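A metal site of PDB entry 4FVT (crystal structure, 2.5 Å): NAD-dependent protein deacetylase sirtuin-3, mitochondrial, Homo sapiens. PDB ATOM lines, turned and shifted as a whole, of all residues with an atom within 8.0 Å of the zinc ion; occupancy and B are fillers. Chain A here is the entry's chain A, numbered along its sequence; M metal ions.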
ATOM      1  N   THR A 134     -22.159 -15.539  15.687  1.00  0.00           N
ATOM      2  CA  THR A 134     -23.576 -15.379  15.997  1.00  0.00           C
ATOM      3  C   THR A 134     -24.079 -14.048  15.475  1.00  0.00           C
ATOM      4  O   THR A 134     -23.371 -13.042  15.528  1.00  0.00           O
ATOM      5  CB  THR A 134     -23.851 -15.468  17.520  1.00  0.00           C
ATOM      6  OG1 THR A 134     -23.389 -16.723  18.016  1.00  0.00           O
ATOM      7  CG2 THR A 134     -25.339 -15.327  17.847  1.00  0.00           C
ATOM      8  N   CYS A 135     -25.312 -14.045  14.987  1.00  0.00           N
ATOM      9  CA  CYS A 135     -25.924 -12.774  14.635  1.00  0.00           C
ATOM     10  C   CYS A 135     -26.241 -11.994  15.916  1.00  0.00           C
ATOM     11  O   CYS A 135     -26.846 -12.533  16.860  1.00  0.00           O
ATOM     12  CB  CYS A 135     -27.180 -12.982  13.798  1.00  0.00           C
ATOM     13  SG  CYS A 135     -28.094 -11.431  13.550  1.00  0.00           S
ATOM     14  N   THR A 136     -25.841 -10.732  15.951  1.00  0.00           N
ATOM     15  CA  THR A 136     -26.027  -9.896  17.121  1.00  0.00           C
ATOM     16  C   THR A 136     -27.497  -9.531  17.313  1.00  0.00           C
ATOM     17  O   THR A 136     -27.905  -9.157  18.394  1.00  0.00           O
ATOM     18  CB  THR A 136     -25.213  -8.610  17.003  1.00  0.00           C
ATOM     19  OG1 THR A 136     -25.587  -7.922  15.798  1.00  0.00           O
ATOM     20  CG2 THR A 136     -23.726  -8.898  16.988  1.00  0.00           C
ATOM     21  N   VAL A 137     -28.282  -9.637  16.250  1.00  0.00           N
ATOM     22  CA  VAL A 137     -29.710  -9.321  16.314  1.00  0.00           C
ATOM     23  C   VAL A 137     -30.607 -10.547  16.615  1.00  0.00           C
ATOM     24  O   VAL A 137     -31.357 -10.542  17.582  1.00  0.00           O
ATOM     25  CB  VAL A 137     -30.197  -8.574  15.033  1.00  0.00           C
ATOM     26  CG1 VAL A 137     -31.712  -8.393  15.038  1.00  0.00           C
ATOM     27  CG2 VAL A 137     -29.485  -7.234  14.898  1.00  0.00           C
ATOM     28  N   CYS A 138     -30.569 -11.563  15.747  1.00  0.00           N
ATOM     29  CA  CYS A 138     -31.485 -12.706  15.873  1.00  0.00           C
ATOM     30  C   CYS A 138     -30.887 -13.920  16.619  1.00  0.00           C
ATOM     31  O   CYS A 138     -31.577 -14.930  16.836  1.00  0.00           O
ATOM     32  CB  CYS A 138     -32.005 -13.136  14.476  1.00  0.00           C
ATOM     33  SG  CYS A 138     -30.754 -13.922  13.369  1.00  0.00           S
ATOM     34  N   GLN A 139     -29.611 -13.835  16.985  1.00  0.00           N
ATOM     35  CA  GLN A 139     -28.965 -14.942  17.685  1.00  0.00           C
ATOM     36  C   GLN A 139     -28.710 -16.236  16.847  1.00  0.00           C
ATOM     37  O   GLN A 139     -28.267 -17.239  17.390  1.00  0.00           O
ATOM     38  CB  GLN A 139     -29.686 -15.277  19.017  1.00  0.00           C
ATOM     39  CG  GLN A 139     -30.226 -14.052  19.790  1.00  0.00           C
ATOM     40  CD  GLN A 139     -29.194 -12.953  19.953  1.00  0.00           C
ATOM     41  OE1 GLN A 139     -28.006 -13.217  20.217  1.00  0.00           O
ATOM     42  NE2 GLN A 139     -29.637 -11.697  19.786  1.00  0.00           N
ATOM     43  N   ARG A 140     -29.066 -16.235  15.554  1.00  0.00           N
ATOM     44  CA  ARG A 140     -28.704 -17.349  14.664  1.00  0.00           C
ATOM     45  C   ARG A 140     -27.199 -17.617  14.641  1.00  0.00           C
ATOM     46  O   ARG A 140     -26.417 -16.678  14.450  1.00  0.00           O
ATOM     47  CB  ARG A 140     -29.213 -17.097  13.241  1.00  0.00           C
ATOM     48  CG  ARG A 140     -30.717 -17.350  13.083  1.00  0.00           C
ATOM     49  CD  ARG A 140     -31.232 -16.996  11.700  1.00  0.00           C
ATOM     50  NE  ARG A 140     -32.642 -17.352  11.541  1.00  0.00           N
ATOM     51  CZ  ARG A 140     -33.653 -16.645  12.038  1.00  0.00           C
ATOM     52  NH1 ARG A 140     -34.914 -17.041  11.839  1.00  0.00           N
ATOM     53  NH2 ARG A 140     -33.414 -15.538  12.741  1.00  0.00           N
ATOM     54  N   PRO A 141     -26.801 -18.876  14.896  1.00  0.00           N
ATOM     55  CA  PRO A 141     -25.406 -19.359  14.861  1.00  0.00           C
ATOM     56  C   PRO A 141     -24.869 -19.685  13.449  1.00  0.00           C
ATOM     57  O   PRO A 141     -25.611 -20.115  12.582  1.00  0.00           O
ATOM     58  CB  PRO A 141     -25.449 -20.624  15.734  1.00  0.00           C
ATOM     59  CG  PRO A 141     -26.854 -21.159  15.511  1.00  0.00           C
ATOM     60  CD  PRO A 141     -27.752 -19.957  15.219  1.00  0.00           C
ATOM     61  N   PHE A 142     -23.580 -19.458  13.249  1.00  0.00           N
ATOM     62  CA  PHE A 142     -22.925 -19.714  11.974  1.00  0.00           C
ATOM     63  C   PHE A 142     -21.526 -20.242  12.221  1.00  0.00           C
ATOM     64  O   PHE A 142     -20.852 -19.805  13.175  1.00  0.00           O
ATOM     65  CB  PHE A 142     -22.794 -18.416  11.155  1.00  0.00           C
ATOM     66  CG  PHE A 142     -24.111 -17.790  10.792  1.00  0.00           C
ATOM     67  CD1 PHE A 142     -24.819 -18.239   9.687  1.00  0.00           C
ATOM     68  CD2 PHE A 142     -24.634 -16.744  11.555  1.00  0.00           C
ATOM     69  CE1 PHE A 142     -26.035 -17.675   9.346  1.00  0.00           C
ATOM     70  CE2 PHE A 142     -25.850 -16.171  11.209  1.00  0.00           C
ATOM     71  CZ  PHE A 142     -26.555 -16.642  10.107  1.00  0.00           C
ATOM     72  N   ARG A 158     -22.821  -9.596   7.536  1.00  0.00           N
ATOM     73  CA  ARG A 158     -24.222  -9.317   7.857  1.00  0.00           C
ATOM     74  C   ARG A 158     -25.070 -10.597   7.799  1.00  0.00           C
ATOM     75  O   ARG A 158     -24.846 -11.479   6.958  1.00  0.00           O
ATOM     76  CB  ARG A 158     -24.768  -8.274   6.882  1.00  0.00           C
ATOM     77  CG  ARG A 158     -24.092  -6.893   6.982  1.00  0.00           C
ATOM     78  CD  ARG A 158     -24.943  -6.006   7.854  1.00  0.00           C
ATOM     79  NE  ARG A 158     -24.298  -4.771   8.256  1.00  0.00           N
ATOM     80  CZ  ARG A 158     -24.861  -3.901   9.102  1.00  0.00           C
ATOM     81  NH1 ARG A 158     -26.050  -4.173   9.626  1.00  0.00           N
ATOM     82  NH2 ARG A 158     -24.220  -2.796   9.441  1.00  0.00           N
ATOM     83  N   CYS A 159     -26.045 -10.698   8.695  1.00  0.00           N
ATOM     84  CA  CYS A 159     -26.925 -11.875   8.769  1.00  0.00           C
ATOM     85  C   CYS A 159     -27.766 -12.048   7.497  1.00  0.00           C
ATOM     86  O   CYS A 159     -28.474 -11.129   7.094  1.00  0.00           O
ATOM     87  CB  CYS A 159     -27.825 -11.748   9.994  1.00  0.00           C
ATOM     88  SG  CYS A 159     -28.988 -13.091  10.232  1.00  0.00           S
ATOM     89  N   PRO A 160     -27.671 -13.219   6.852  1.00  0.00           N
ATOM     90  CA  PRO A 160     -28.483 -13.486   5.653  1.00  0.00           C
ATOM     91  C   PRO A 160     -29.984 -13.475   5.902  1.00  0.00           C
ATOM     92  O   PRO A 160     -30.739 -13.231   4.984  1.00  0.00           O
ATOM     93  CB  PRO A 160     -28.025 -14.879   5.206  1.00  0.00           C
ATOM     94  CG  PRO A 160     -27.242 -15.441   6.349  1.00  0.00           C
ATOM     95  CD  PRO A 160     -26.658 -14.274   7.079  1.00  0.00           C
ATOM     96  N   VAL A 161     -30.413 -13.691   7.141  1.00  0.00           N
ATOM     97  CA  VAL A 161     -31.851 -13.674   7.443  1.00  0.00           C
ATOM     98  C   VAL A 161     -32.412 -12.286   7.825  1.00  0.00           C
ATOM     99  O   VAL A 161     -33.393 -11.836   7.209  1.00  0.00           O
ATOM    100  CB  VAL A 161     -32.245 -14.733   8.494  1.00  0.00           C
ATOM    101  CG1 VAL A 161     -33.738 -14.743   8.660  1.00  0.00           C
ATOM    102  CG2 VAL A 161     -31.747 -16.103   8.093  1.00  0.00           C
ATOM    103  N   CYS A 162     -31.865 -11.670   8.892  1.00  0.00           N
ATOM    104  CA  CYS A 162     -32.239 -10.323   9.384  1.00  0.00           C
ATOM    105  C   CYS A 162     -31.320  -9.103   9.018  1.00  0.00           C
ATOM    106  O   CYS A 162     -31.641  -7.976   9.401  1.00  0.00           O
ATOM    107  CB  CYS A 162     -32.455 -10.346  10.905  1.00  0.00           C
ATOM    108  SG  CYS A 162     -30.938 -10.263  11.882  1.00  0.00           S
ATOM    109  N   THR A 163     -30.214  -9.333   8.300  1.00  0.00           N
ATOM    110  CA  THR A 163     -29.219  -8.282   7.998  1.00  0.00           C
ATOM    111  C   THR A 163     -28.414  -7.766   9.187  1.00  0.00           C
ATOM    112  O   THR A 163     -27.565  -6.875   9.024  1.00  0.00           O
ATOM    113  CB  THR A 163     -29.769  -7.047   7.190  1.00  0.00           C
ATOM    114  OG1 THR A 163     -30.635  -6.252   8.020  1.00  0.00           O
ATOM    115  CG2 THR A 163     -30.472  -7.479   5.899  1.00  0.00           C
ATOM    116  N   GLY A 164     -28.684  -8.278  10.389  1.00  0.00           N
ATOM    117  CA  GLY A 164     -27.868  -7.936  11.538  1.00  0.00           C
ATOM    118  C   GLY A 164     -26.388  -8.269  11.427  1.00  0.00           C
ATOM    119  O   GLY A 164     -25.988  -9.205  10.714  1.00  0.00           O
ATOM    120  N   VAL A 165     -25.541  -7.507  12.124  1.00  0.00           N
ATOM    121  CA  VAL A 165     -24.116  -7.761  12.130  1.00  0.00           C
ATOM    122  C   VAL A 165     -23.798  -9.131  12.760  1.00  0.00           C
ATOM    123  O   VAL A 165     -24.260  -9.434  13.862  1.00  0.00           O
ATOM    124  CB  VAL A 165     -23.346  -6.667  12.890  1.00  0.00           C
ATOM    125  CG1 VAL A 165     -21.919  -7.126  13.198  1.00  0.00           C
ATOM    126  CG2 VAL A 165     -23.344  -5.357  12.086  1.00  0.00           C
ATOM    127  N   VAL A 166     -23.013  -9.945  12.068  1.00  0.00           N
ATOM    128  CA  VAL A 166     -22.637 -11.261  12.592  1.00  0.00           C
ATOM    129  C   VAL A 166     -21.295 -11.185  13.320  1.00  0.00           C
ATOM    130  O   VAL A 166     -20.281 -10.819  12.742  1.00  0.00           O
ATOM    131  CB  VAL A 166     -22.618 -12.354  11.496  1.00  0.00           C
ATOM    132  CG1 VAL A 166     -22.100 -13.689  12.062  1.00  0.00           C
ATOM    133  CG2 VAL A 166     -24.008 -12.532  10.872  1.00  0.00           C
HETATM  134 ZN    ZN M   1     -29.861 -12.275  12.205  1.00  0.00          ZN
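The backbone carbonyl oxygen (O) of Gly 164 sits at hydrogen-bond distance from the backbone NH (N) of Cys 159 (2.5 Å). The side-chain sulfur of Cys 159 lies close to the backbone NH of Val 161 (3.5 Å). The backbone NH (N) of Cys 135 lies within hydrogen-bond range of the backbone carbonyl oxygen (O) of Arg 140 (2.9 Å). The side-chain sulfur (SG) of Cys 162 sits close to the backbone NH (N) of Gly 164 (3.4 Å). The side-chain sulfur of Cys 135 lies close to the backbone NH of Val 137, at 3.2 Å. SG of Cys 138 sits close to NH2 of Arg 140, 3.2 Å away.
The side-chain sulfur (SG) of Cys 138 is bound to the zinc ion, 2.2 Å away. SG of Cys 162 binds the zinc ion, 2.3 Å away. SG of Cys 159 is bound to the zinc ion, at 2.3 Å. The side-chain sulfur (SG) of Cys 135 is bound to the zinc ion, 2.4 Å away.
The nearest printed residue that does not touch the zinc ion is Gly 164 (4.5 Å).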
